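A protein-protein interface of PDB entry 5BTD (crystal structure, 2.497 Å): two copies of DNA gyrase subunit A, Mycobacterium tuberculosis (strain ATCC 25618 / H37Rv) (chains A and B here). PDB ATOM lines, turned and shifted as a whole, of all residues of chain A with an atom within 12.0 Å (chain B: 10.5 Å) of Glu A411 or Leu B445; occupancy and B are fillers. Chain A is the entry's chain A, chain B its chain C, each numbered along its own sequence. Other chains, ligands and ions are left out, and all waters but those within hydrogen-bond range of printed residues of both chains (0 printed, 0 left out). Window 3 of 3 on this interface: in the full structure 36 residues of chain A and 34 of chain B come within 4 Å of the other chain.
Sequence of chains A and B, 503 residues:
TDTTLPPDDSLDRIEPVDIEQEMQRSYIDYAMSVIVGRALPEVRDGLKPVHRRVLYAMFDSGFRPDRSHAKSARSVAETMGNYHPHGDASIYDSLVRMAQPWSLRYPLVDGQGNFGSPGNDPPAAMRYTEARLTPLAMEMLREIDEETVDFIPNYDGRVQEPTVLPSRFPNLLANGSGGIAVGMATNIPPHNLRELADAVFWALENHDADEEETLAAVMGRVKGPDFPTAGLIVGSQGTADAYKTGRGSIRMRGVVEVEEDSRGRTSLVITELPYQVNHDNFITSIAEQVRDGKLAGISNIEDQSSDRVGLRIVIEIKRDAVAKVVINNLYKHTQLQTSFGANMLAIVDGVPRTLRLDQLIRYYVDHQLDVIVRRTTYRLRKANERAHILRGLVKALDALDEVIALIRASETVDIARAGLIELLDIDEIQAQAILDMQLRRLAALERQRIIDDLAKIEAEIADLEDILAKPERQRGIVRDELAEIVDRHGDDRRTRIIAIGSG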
ATOM      1  N   VAL A 403      14.752  -8.540  20.822  1.00  0.00           N
ATOM      2  CA  VAL A 403      15.951  -9.316  21.124  1.00  0.00           C
ATOM      3  C   VAL A 403      15.651 -10.810  21.241  1.00  0.00           C
ATOM      4  O   VAL A 403      16.344 -11.639  20.652  1.00  0.00           O
ATOM      5  CB  VAL A 403      16.614  -8.824  22.438  1.00  0.00           C
ATOM      6  CG1 VAL A 403      17.693  -9.800  22.918  1.00  0.00           C
ATOM      7  CG2 VAL A 403      17.205  -7.439  22.253  1.00  0.00           C
ATOM      8  N   ILE A 404      14.619 -11.146  22.005  1.00  0.00           N
ATOM      9  CA  ILE A 404      14.277 -12.539  22.256  1.00  0.00           C
ATOM     10  C   ILE A 404      13.807 -13.260  20.997  1.00  0.00           C
ATOM     11  O   ILE A 404      14.281 -14.356  20.696  1.00  0.00           O
ATOM     12  CB  ILE A 404      13.183 -12.647  23.332  1.00  0.00           C
ATOM     13  CG1 ILE A 404      13.680 -12.015  24.635  1.00  0.00           C
ATOM     14  CG2 ILE A 404      12.772 -14.111  23.546  1.00  0.00           C
ATOM     15  CD1 ILE A 404      12.644 -11.944  25.721  1.00  0.00           C
ATOM     16  N   ALA A 405      12.884 -12.643  20.265  1.00  0.00           N
ATOM     17  CA  ALA A 405      12.343 -13.241  19.047  1.00  0.00           C
ATOM     18  C   ALA A 405      13.444 -13.598  18.053  1.00  0.00           C
ATOM     19  O   ALA A 405      13.378 -14.632  17.383  1.00  0.00           O
ATOM     20  CB  ALA A 405      11.342 -12.299  18.401  1.00  0.00           C
ATOM     21  N   LEU A 406      14.458 -12.743  17.975  1.00  0.00           N
ATOM     22  CA  LEU A 406      15.567 -12.938  17.046  1.00  0.00           C
ATOM     23  C   LEU A 406      16.392 -14.172  17.392  1.00  0.00           C
ATOM     24  O   LEU A 406      16.701 -14.991  16.528  1.00  0.00           O
ATOM     25  CB  LEU A 406      16.461 -11.701  17.039  1.00  0.00           C
ATOM     26  CG  LEU A 406      17.770 -11.815  16.260  1.00  0.00           C
ATOM     27  CD1 LEU A 406      17.509 -11.966  14.761  1.00  0.00           C
ATOM     28  CD2 LEU A 406      18.622 -10.605  16.537  1.00  0.00           C
ATOM     29  N   ILE A 407      16.745 -14.293  18.666  1.00  0.00           N
ATOM     30  CA  ILE A 407      17.577 -15.394  19.133  1.00  0.00           C
ATOM     31  C   ILE A 407      16.870 -16.727  18.904  1.00  0.00           C
ATOM     32  O   ILE A 407      17.507 -17.725  18.571  1.00  0.00           O
ATOM     33  CB  ILE A 407      17.935 -15.228  20.626  1.00  0.00           C
ATOM     34  CG1 ILE A 407      18.765 -13.956  20.821  1.00  0.00           C
ATOM     35  CG2 ILE A 407      18.699 -16.447  21.142  1.00  0.00           C
ATOM     36  CD1 ILE A 407      19.029 -13.591  22.264  1.00  0.00           C
ATOM     37  N   ARG A 408      15.552 -16.730  19.072  1.00  0.00           N
ATOM     38  CA  ARG A 408      14.753 -17.947  18.940  1.00  0.00           C
ATOM     39  C   ARG A 408      14.883 -18.597  17.564  1.00  0.00           C
ATOM     40  O   ARG A 408      15.079 -19.809  17.460  1.00  0.00           O
ATOM     41  CB  ARG A 408      13.279 -17.628  19.194  1.00  0.00           C
ATOM     42  CG  ARG A 408      12.965 -17.158  20.606  1.00  0.00           C
ATOM     43  CD  ARG A 408      12.564 -18.288  21.531  1.00  0.00           C
ATOM     44  NE  ARG A 408      11.554 -17.853  22.496  1.00  0.00           N
ATOM     45  CZ  ARG A 408      10.238 -17.961  22.319  1.00  0.00           C
ATOM     46  NH1 ARG A 408       9.742 -18.498  21.211  1.00  0.00           N
ATOM     47  NH2 ARG A 408       9.411 -17.532  23.262  1.00  0.00           N
ATOM     48  N   ALA A 409      14.784 -17.787  16.516  1.00  0.00           N
ATOM     49  CA  ALA A 409      14.742 -18.290  15.144  1.00  0.00           C
ATOM     50  C   ALA A 409      16.110 -18.693  14.592  1.00  0.00           C
ATOM     51  O   ALA A 409      16.216 -19.097  13.433  1.00  0.00           O
ATOM     52  CB  ALA A 409      14.111 -17.248  14.236  1.00  0.00           C
ATOM     53  N   SER A 410      17.152 -18.588  15.411  1.00  0.00           N
ATOM     54  CA  SER A 410      18.506 -18.881  14.949  1.00  0.00           C
ATOM     55  C   SER A 410      18.893 -20.355  15.095  1.00  0.00           C
ATOM     56  O   SER A 410      18.684 -20.967  16.145  1.00  0.00           O
ATOM     57  CB  SER A 410      19.508 -18.009  15.709  1.00  0.00           C
ATOM     58  OG  SER A 410      19.182 -16.636  15.580  1.00  0.00           O
ATOM     59  N   GLU A 411      19.470 -20.907  14.030  1.00  0.00           N
ATOM     60  CA  GLU A 411      19.917 -22.298  14.017  1.00  0.00           C
ATOM     61  C   GLU A 411      21.118 -22.462  14.944  1.00  0.00           C
ATOM     62  O   GLU A 411      21.295 -23.507  15.560  1.00  0.00           O
ATOM     63  CB  GLU A 411      20.279 -22.745  12.593  1.00  0.00           C
ATOM     64  CG  GLU A 411      19.085 -22.925  11.660  1.00  0.00           C
ATOM     65  CD  GLU A 411      19.481 -23.434  10.282  1.00  0.00           C
ATOM     66  OE1 GLU A 411      20.697 -23.554  10.015  1.00  0.00           O
ATOM     67  OE2 GLU A 411      18.578 -23.712   9.464  1.00  0.00           O
ATOM     68  N   THR A 412      21.943 -21.424  15.025  1.00  0.00           N
ATOM     69  CA  THR A 412      23.083 -21.410  15.934  1.00  0.00           C
ATOM     70  C   THR A 412      22.983 -20.175  16.815  1.00  0.00           C
ATOM     71  O   THR A 412      21.988 -19.452  16.769  1.00  0.00           O
ATOM     72  CB  THR A 412      24.433 -21.395  15.186  1.00  0.00           C
ATOM     73  OG1 THR A 412      24.666 -20.094  14.632  1.00  0.00           O
ATOM     74  CG2 THR A 412      24.458 -22.438  14.076  1.00  0.00           C
ATOM     75  N   VAL A 413      24.012 -19.939  17.619  1.00  0.00           N
ATOM     76  CA  VAL A 413      24.086 -18.725  18.418  1.00  0.00           C
ATOM     77  C   VAL A 413      24.740 -17.632  17.582  1.00  0.00           C
ATOM     78  O   VAL A 413      24.555 -16.441  17.837  1.00  0.00           O
ATOM     79  CB  VAL A 413      24.883 -18.931  19.724  1.00  0.00           C
ATOM     80  CG1 VAL A 413      24.187 -19.951  20.612  1.00  0.00           C
ATOM     81  CG2 VAL A 413      26.321 -19.357  19.429  1.00  0.00           C
ATOM     82  N   ASP A 414      25.504 -18.051  16.578  1.00  0.00           N
ATOM     83  CA  ASP A 414      26.178 -17.125  15.679  1.00  0.00           C
ATOM     84  C   ASP A 414      25.175 -16.360  14.818  1.00  0.00           C
ATOM     85  O   ASP A 414      25.334 -15.158  14.596  1.00  0.00           O
ATOM     86  CB  ASP A 414      27.171 -17.881  14.794  1.00  0.00           C
ATOM     87  CG  ASP A 414      28.170 -18.692  15.603  1.00  0.00           C
ATOM     88  OD1 ASP A 414      28.618 -18.201  16.659  1.00  0.00           O
ATOM     89  OD2 ASP A 414      28.501 -19.822  15.187  1.00  0.00           O
ATOM     90  N   ILE A 415      24.150 -17.053  14.327  1.00  0.00           N
ATOM     91  CA  ILE A 415      23.085 -16.396  13.573  1.00  0.00           C
ATOM     92  C   ILE A 415      22.346 -15.418  14.485  1.00  0.00           C
ATOM     93  O   ILE A 415      21.993 -14.312  14.070  1.00  0.00           O
ATOM     94  CB  ILE A 415      22.090 -17.417  12.955  1.00  0.00           C
ATOM     95  CG1 ILE A 415      22.692 -18.089  11.718  1.00  0.00           C
ATOM     96  CG2 ILE A 415      20.800 -16.730  12.502  1.00  0.00           C
ATOM     97  CD1 ILE A 415      23.782 -19.097  11.994  1.00  0.00           C
ATOM     98  N   ALA A 416      22.116 -15.829  15.726  1.00  0.00           N
ATOM     99  CA  ALA A 416      21.465 -14.967  16.705  1.00  0.00           C
ATOM    100  C   ALA A 416      22.295 -13.718  16.977  1.00  0.00           C
ATOM    101  O   ALA A 416      21.760 -12.611  17.029  1.00  0.00           O
ATOM    102  CB  ALA A 416      21.217 -15.725  17.994  1.00  0.00           C
ATOM    103  N   ARG A 417      23.601 -13.899  17.158  1.00  0.00           N
ATOM    104  CA  ARG A 417      24.492 -12.774  17.422  1.00  0.00           C
ATOM    105  C   ARG A 417      24.521 -11.816  16.239  1.00  0.00           C
ATOM    106  O   ARG A 417      24.209 -10.636  16.387  1.00  0.00           O
ATOM    107  CB  ARG A 417      25.911 -13.252  17.737  1.00  0.00           C
ATOM    108  CG  ARG A 417      26.758 -12.164  18.394  1.00  0.00           C
ATOM    109  CD  ARG A 417      28.129 -12.649  18.845  1.00  0.00           C
ATOM    110  NE  ARG A 417      28.791 -13.477  17.841  1.00  0.00           N
ATOM    111  CZ  ARG A 417      28.823 -14.807  17.848  1.00  0.00           C
ATOM    112  NH1 ARG A 417      28.231 -15.501  18.813  1.00  0.00           N
ATOM    113  NH2 ARG A 417      29.456 -15.449  16.876  1.00  0.00           N
ATOM    114  N   ALA A 418      24.899 -12.333  15.070  1.00  0.00           N
ATOM    115  CA  ALA A 418      24.968 -11.536  13.848  1.00  0.00           C
ATOM    116  C   ALA A 418      23.716 -10.687  13.670  1.00  0.00           C
ATOM    117  O   ALA A 418      23.791  -9.543  13.227  1.00  0.00           O
ATOM    118  CB  ALA A 418      25.173 -12.435  12.638  1.00  0.00           C
ATOM    119  N   GLY A 419      22.568 -11.248  14.037  1.00  0.00           N
ATOM    120  CA  GLY A 419      21.315 -10.517  13.988  1.00  0.00           C
ATOM    121  C   GLY A 419      21.278  -9.364  14.975  1.00  0.00           C
ATOM    122  O   GLY A 419      20.791  -8.280  14.655  1.00  0.00           O
ATOM    123  N   LEU A 420      21.767  -9.611  16.189  1.00  0.00           N
ATOM    124  CA  LEU A 420      21.781  -8.593  17.235  1.00  0.00           C
ATOM    125  C   LEU A 420      22.609  -7.385  16.807  1.00  0.00           C
ATOM    126  O   LEU A 420      22.240  -6.242  17.081  1.00  0.00           O
ATOM    127  CB  LEU A 420      22.327  -9.170  18.544  1.00  0.00           C
ATOM    128  CG  LEU A 420      21.419 -10.174  19.259  1.00  0.00           C
ATOM    129  CD1 LEU A 420      22.210 -11.011  20.261  1.00  0.00           C
ATOM    130  CD2 LEU A 420      20.270  -9.460  19.951  1.00  0.00           C
ATOM    131  N   LEU A 435      24.178 -12.084  24.867  1.00  0.00           N
ATOM    132  CA  LEU A 435      23.971 -13.525  24.767  1.00  0.00           C
ATOM    133  C   LEU A 435      24.242 -14.221  26.096  1.00  0.00           C
ATOM    134  O   LEU A 435      23.511 -15.131  26.492  1.00  0.00           O
ATOM    135  CB  LEU A 435      24.872 -14.110  23.676  1.00  0.00           C
ATOM    136  CG  LEU A 435      24.422 -13.927  22.227  1.00  0.00           C
ATOM    137  CD1 LEU A 435      25.534 -14.343  21.282  1.00  0.00           C
ATOM    138  CD2 LEU A 435      23.162 -14.729  21.944  1.00  0.00           C
ATOM    139  N   LEU B 397      10.584 -24.204  28.607  1.00  0.00           N
ATOM    140  CA  LEU B 397      10.600 -24.049  27.155  1.00  0.00           C
ATOM    141  C   LEU B 397       9.214 -24.241  26.541  1.00  0.00           C
ATOM    142  O   LEU B 397       8.838 -23.531  25.608  1.00  0.00           O
ATOM    143  CB  LEU B 397      11.583 -25.041  26.532  1.00  0.00           C
ATOM    144  CG  LEU B 397      13.055 -24.875  26.920  1.00  0.00           C
ATOM    145  CD1 LEU B 397      13.900 -25.975  26.293  1.00  0.00           C
ATOM    146  CD2 LEU B 397      13.588 -23.501  26.529  1.00  0.00           C
ATOM    147  N   LEU B 439      20.391 -16.267  27.867  1.00  0.00           N
ATOM    148  CA  LEU B 439      19.614 -16.028  26.652  1.00  0.00           C
ATOM    149  C   LEU B 439      20.136 -16.877  25.499  1.00  0.00           C
ATOM    150  O   LEU B 439      19.406 -17.166  24.553  1.00  0.00           O
ATOM    151  CB  LEU B 439      19.650 -14.545  26.268  1.00  0.00           C
ATOM    152  CG  LEU B 439      19.014 -13.562  27.256  1.00  0.00           C
ATOM    153  CD1 LEU B 439      19.120 -12.140  26.729  1.00  0.00           C
ATOM    154  CD2 LEU B 439      17.560 -13.912  27.536  1.00  0.00           C
ATOM    155  N   ARG B 440      21.405 -17.265  25.583  1.00  0.00           N
ATOM    156  CA  ARG B 440      21.992 -18.200  24.630  1.00  0.00           C
ATOM    157  C   ARG B 440      21.141 -19.452  24.463  1.00  0.00           C
ATOM    158  O   ARG B 440      20.919 -19.921  23.348  1.00  0.00           O
ATOM    159  CB  ARG B 440      23.400 -18.604  25.065  1.00  0.00           C
ATOM    160  CG  ARG B 440      24.496 -17.792  24.423  1.00  0.00           C
ATOM    161  CD  ARG B 440      25.863 -18.295  24.843  1.00  0.00           C
ATOM    162  NE  ARG B 440      26.926 -17.695  24.037  1.00  0.00           N
ATOM    163  CZ  ARG B 440      27.970 -18.358  23.537  1.00  0.00           C
ATOM    164  NH1 ARG B 440      28.124 -19.660  23.755  1.00  0.00           N
ATOM    165  NH2 ARG B 440      28.872 -17.710  22.813  1.00  0.00           N
ATOM    166  N   ARG B 441      20.659 -19.981  25.582  1.00  0.00           N
ATOM    167  CA  ARG B 441      19.991 -21.273  25.588  1.00  0.00           C
ATOM    168  C   ARG B 441      18.577 -21.198  25.004  1.00  0.00           C
ATOM    169  O   ARG B 441      17.882 -22.212  24.918  1.00  0.00           O
ATOM    170  CB  ARG B 441      19.931 -21.816  27.019  1.00  0.00           C
ATOM    171  CG  ARG B 441      21.270 -22.297  27.570  1.00  0.00           C
ATOM    172  CD  ARG B 441      21.098 -22.942  28.938  1.00  0.00           C
ATOM    173  NE  ARG B 441      22.364 -23.088  29.653  1.00  0.00           N
ATOM    174  CZ  ARG B 441      22.464 -23.368  30.951  1.00  0.00           C
ATOM    175  NH1 ARG B 441      21.373 -23.537  31.689  1.00  0.00           N
ATOM    176  NH2 ARG B 441      23.660 -23.481  31.517  1.00  0.00           N
ATOM    177  N   LEU B 442      18.160 -20.001  24.596  1.00  0.00           N
ATOM    178  CA  LEU B 442      16.841 -19.811  24.001  1.00  0.00           C
ATOM    179  C   LEU B 442      16.864 -19.956  22.479  1.00  0.00           C
ATOM    180  O   LEU B 442      15.815 -19.906  21.834  1.00  0.00           O
ATOM    181  CB  LEU B 442      16.279 -18.438  24.381  1.00  0.00           C
ATOM    182  CG  LEU B 442      16.015 -18.197  25.870  1.00  0.00           C
ATOM    183  CD1 LEU B 442      15.411 -16.817  26.084  1.00  0.00           C
ATOM    184  CD2 LEU B 442      15.112 -19.271  26.465  1.00  0.00           C
ATOM    185  N   ALA B 443      18.050 -20.138  21.904  1.00  0.00           N
ATOM    186  CA  ALA B 443      18.161 -20.374  20.467  1.00  0.00           C
ATOM    187  C   ALA B 443      17.575 -21.736  20.113  1.00  0.00           C
ATOM    188  O   ALA B 443      17.524 -22.629  20.957  1.00  0.00           O
ATOM    189  CB  ALA B 443      19.611 -20.286  20.017  1.00  0.00           C
ATOM    190  N   ALA B 444      17.135 -21.886  18.866  1.00  0.00           N
ATOM    191  CA  ALA B 444      16.443 -23.098  18.432  1.00  0.00           C
ATOM    192  C   ALA B 444      17.256 -24.352  18.746  1.00  0.00           C
ATOM    193  O   ALA B 444      16.785 -25.246  19.451  1.00  0.00           O
ATOM    194  CB  ALA B 444      16.141 -23.028  16.945  1.00  0.00           C
ATOM    195  N   LEU B 445      18.478 -24.410  18.225  1.00  0.00           N
ATOM    196  CA  LEU B 445      19.338 -25.572  18.425  1.00  0.00           C
ATOM    197  C   LEU B 445      19.702 -25.745  19.893  1.00  0.00           C
ATOM    198  O   LEU B 445      19.926 -26.861  20.360  1.00  0.00           O
ATOM    199  CB  LEU B 445      20.608 -25.443  17.586  1.00  0.00           C
ATOM    200  CG  LEU B 445      21.686 -26.514  17.760  1.00  0.00           C
ATOM    201  CD1 LEU B 445      21.127 -27.896  17.468  1.00  0.00           C
ATOM    202  CD2 LEU B 445      22.874 -26.218  16.861  1.00  0.00           C
ATOM    203  N   GLU B 446      19.763 -24.635  20.619  1.00  0.00           N
ATOM    204  CA  GLU B 446      20.127 -24.672  22.029  1.00  0.00           C
ATOM    205  C   GLU B 446      18.986 -25.222  22.882  1.00  0.00           C
ATOM    206  O   GLU B 446      19.224 -25.902  23.881  1.00  0.00           O
ATOM    207  CB  GLU B 446      20.534 -23.281  22.508  1.00  0.00           C
ATOM    208  CG  GLU B 446      21.783 -22.753  21.817  1.00  0.00           C
ATOM    209  CD  GLU B 446      23.021 -23.577  22.122  1.00  0.00           C
ATOM    210  OE1 GLU B 446      22.979 -24.408  23.055  1.00  0.00           O
ATOM    211  OE2 GLU B 446      24.040 -23.396  21.422  1.00  0.00           O
ATOM    212  N   ARG B 447      17.752 -24.908  22.500  1.00  0.00           N
ATOM    213  CA  ARG B 447      16.586 -25.503  23.144  1.00  0.00           C
ATOM    214  C   ARG B 447      16.615 -27.015  22.941  1.00  0.00           C
ATOM    215  O   ARG B 447      16.301 -27.786  23.849  1.00  0.00           O
ATOM    216  CB  ARG B 447      15.278 -24.933  22.580  1.00  0.00           C
ATOM    217  CG  ARG B 447      14.997 -23.478  22.931  1.00  0.00           C
ATOM    218  CD  ARG B 447      13.595 -23.049  22.493  1.00  0.00           C
ATOM    219  NE  ARG B 447      13.056 -23.891  21.421  1.00  0.00           N
ATOM    220  CZ  ARG B 447      12.129 -24.839  21.578  1.00  0.00           C
ATOM    221  NH1 ARG B 447      11.608 -25.101  22.772  1.00  0.00           N
ATOM    222  NH2 ARG B 447      11.719 -25.538  20.527  1.00  0.00           N
ATOM    223  N   GLN B 448      17.010 -27.426  21.739  1.00  0.00           N
ATOM    224  CA  GLN B 448      17.038 -28.835  21.363  1.00  0.00           C
ATOM    225  C   GLN B 448      18.064 -29.635  22.166  1.00  0.00           C
ATOM    226  O   GLN B 448      17.831 -30.796  22.496  1.00  0.00           O
ATOM    227  CB  GLN B 448      17.339 -28.966  19.864  1.00  0.00           C
ATOM    228  CG  GLN B 448      17.269 -30.385  19.324  1.00  0.00           C
ATOM    229  CD  GLN B 448      15.890 -30.996  19.480  1.00  0.00           C
ATOM    230  OE1 GLN B 448      15.706 -31.972  20.209  1.00  0.00           O
ATOM    231  NE2 GLN B 448      14.909 -30.421  18.793  1.00  0.00           N
ATOM    232  N   ARG B 449      19.199 -29.018  22.478  1.00  0.00           N
ATOM    233  CA  ARG B 449      20.243 -29.703  23.230  1.00  0.00           C
ATOM    234  C   ARG B 449      19.777 -30.035  24.644  1.00  0.00           C
ATOM    235  O   ARG B 449      20.145 -31.072  25.194  1.00  0.00           O
ATOM    236  CB  ARG B 449      21.520 -28.866  23.283  1.00  0.00           C
ATOM    237  CG  ARG B 449      22.663 -29.582  23.983  1.00  0.00           C
ATOM    238  CD  ARG B 449      23.997 -28.886  23.773  1.00  0.00           C
ATOM    239  NE  ARG B 449      24.417 -28.911  22.375  1.00  0.00           N
ATOM    240  CZ  ARG B 449      25.445 -28.223  21.886  1.00  0.00           C
ATOM    241  NH1 ARG B 449      26.177 -27.454  22.683  1.00  0.00           N
ATOM    242  NH2 ARG B 449      25.750 -28.312  20.599  1.00  0.00           N
ATOM    243  N   ILE B 450      18.978 -29.149  25.231  1.00  0.00           N
ATOM    244  CA  ILE B 450      18.409 -29.392  26.552  1.00  0.00           C
ATOM    245  C   ILE B 450      17.533 -30.643  26.521  1.00  0.00           C
ATOM    246  O   ILE B 450      17.623 -31.499  27.406  1.00  0.00           O
ATOM    247  CB  ILE B 450      17.584 -28.179  27.042  1.00  0.00           C
ATOM    248  CG1 ILE B 450      18.503 -26.971  27.237  1.00  0.00           C
ATOM    249  CG2 ILE B 450      16.847 -28.502  28.346  1.00  0.00           C
ATOM    250  CD1 ILE B 450      17.774 -25.667  27.488  1.00  0.00           C
ATOM    251  N   ILE B 451      16.690 -30.740  25.497  1.00  0.00           N
ATOM    252  CA  ILE B 451      15.845 -31.913  25.306  1.00  0.00           C
ATOM    253  C   ILE B 451      16.703 -33.170  25.187  1.00  0.00           C
ATOM    254  O   ILE B 451      16.530 -34.124  25.946  1.00  0.00           O
ATOM    255  CB  ILE B 451      14.956 -31.777  24.047  1.00  0.00           C
ATOM    256  CG1 ILE B 451      14.080 -30.523  24.138  1.00  0.00           C
ATOM    257  CG2 ILE B 451      14.106 -33.034  23.838  1.00  0.00           C
ATOM    258  CD1 ILE B 451      13.045 -30.560  25.241  1.00  0.00           C
ATOM    259  N   ASP B 452      17.631 -33.161  24.234  1.00  0.00           N
ATOM    260  CA  ASP B 452      18.490 -34.313  23.985  1.00  0.00           C
ATOM    261  C   ASP B 452      19.325 -34.670  25.211  1.00  0.00           C
ATOM    262  O   ASP B 452      19.531 -35.846  25.505  1.00  0.00           O
ATOM    263  CB  ASP B 452      19.413 -34.044  22.793  1.00  0.00           C
ATOM    264  CG  ASP B 452      18.655 -33.907  21.486  1.00  0.00           C
ATOM    265  OD1 ASP B 452      17.587 -34.540  21.341  1.00  0.00           O
ATOM    266  OD2 ASP B 452      19.129 -33.162  20.603  1.00  0.00           O
ATOM    267  N   ASP B 453      19.798 -33.656  25.929  1.00  0.00           N
ATOM    268  CA  ASP B 453      20.587 -33.882  27.134  1.00  0.00           C
ATOM    269  C   ASP B 453      19.765 -34.622  28.180  1.00  0.00           C
ATOM    270  O   ASP B 453      20.272 -35.515  28.859  1.00  0.00           O
ATOM    271  CB  ASP B 453      21.110 -32.560  27.700  1.00  0.00           C
ATOM    272  CG  ASP B 453      22.356 -32.066  26.978  1.00  0.00           C
ATOM    273  OD1 ASP B 453      22.671 -32.598  25.892  1.00  0.00           O
ATOM    274  OD2 ASP B 453      23.025 -31.145  27.494  1.00  0.00           O
ATOM    275  N   LYS B 456      19.606 -37.984  26.976  1.00  0.00           N
ATOM    276  CA  LYS B 456      20.936 -38.556  27.157  1.00  0.00           C
ATOM    277  C   LYS B 456      21.142 -39.029  28.594  1.00  0.00           C
ATOM    278  O   LYS B 456      21.564 -40.161  28.830  1.00  0.00           O
ATOM    279  CB  LYS B 456      22.009 -37.526  26.795  1.00  0.00           C
ATOM    280  CG  LYS B 456      22.271 -37.352  25.303  1.00  0.00           C
ATOM    281  CD  LYS B 456      23.267 -36.222  25.058  1.00  0.00           C
ATOM    282  CE  LYS B 456      23.505 -35.989  23.577  1.00  0.00           C
ATOM    283  NZ  LYS B 456      24.462 -34.872  23.341  1.00  0.00           N
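Of the 19 printed residues of chain A, 6 touch a printed residue of chain B.
Hydrophobic or aromatic side chains of chain A within 4 Å of the printed part of chain B: Ile A407, Val A413 and Leu A435.
Of the 17 printed residues of chain B, 7 touch a printed residue of chain A.
Hydrophobic or aromatic side chains of chain B that line the printed part of chain A: Leu B439, Ala B443, Ala B444 and Leu B445.
Among the printed residues, 9 pairs touch across the chains.
Among the printed residues, no Asp or Glu carboxylate lies within 4 Å of a Lys or Arg side-chain nitrogen of the other chain.
Ala A405 touches none of the printed residues of chain B.
Of chain B, only Ala B444 (3.3 Å) comes within 4 Å of Ser A410.
Glu A411 touches just one residue of chain B: Leu B445.
Gly A419 touches none of the printed residues of chain B.
Printed residues of chain B within 4 Å of Leu A435: Leu B439 and Arg B440.
Of the printed residues of chain A, Leu B439 touches Ile A407 (3.6 Å) and Leu A435 (3.6 Å).
Ala B443 touches just one residue of chain A: Ile A407.
Of chain A, only Glu A411 comes within 4 Å of Leu B445.
The backbone carbonyl oxygen of Arg A408 lies within hydrogen-bond range of the backbone NH of Ala B444 (3.2 Å).
The backbone carbonyl oxygen (O) of Leu A435 lies within hydrogen-bond range of the backbone NH (N) of Arg B440.
The backbone carbonyl oxygen (O) of Ser A410 is in hydrogen-bond range of the backbone NH (N) of Ala B444, 3.3 Å away.
The backbone carbonyl oxygen (O) of Leu A406 lies within hydrogen-bond range of the side-chain hydroxyl (OG) of Ser A410, at 3.1 Å.
The side-chain hydroxyl (OG) of Ser A410 sits close to the backbone NH (N) of Ala A416 (3.0 Å).
No position is printed for both chains.
Of the 9 pairs that touch across the chains among the printed residues, none has its exchanged pair printed and touching as well.
Ile A407 touches Leu B439.
Ile A407 touches Ala B443 (O to CA, 3.3 Å).
Arg A408 touches Leu B442 (CD to O, 3.6 Å).
Glu A411 touches Leu B445 (O to CB, 2.9 Å).
Val A413 touches Glu B446 (CG1 to OE2, 3.5 Å).
Leu A435 touches Leu B439 (O to N, 3.6 Å).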
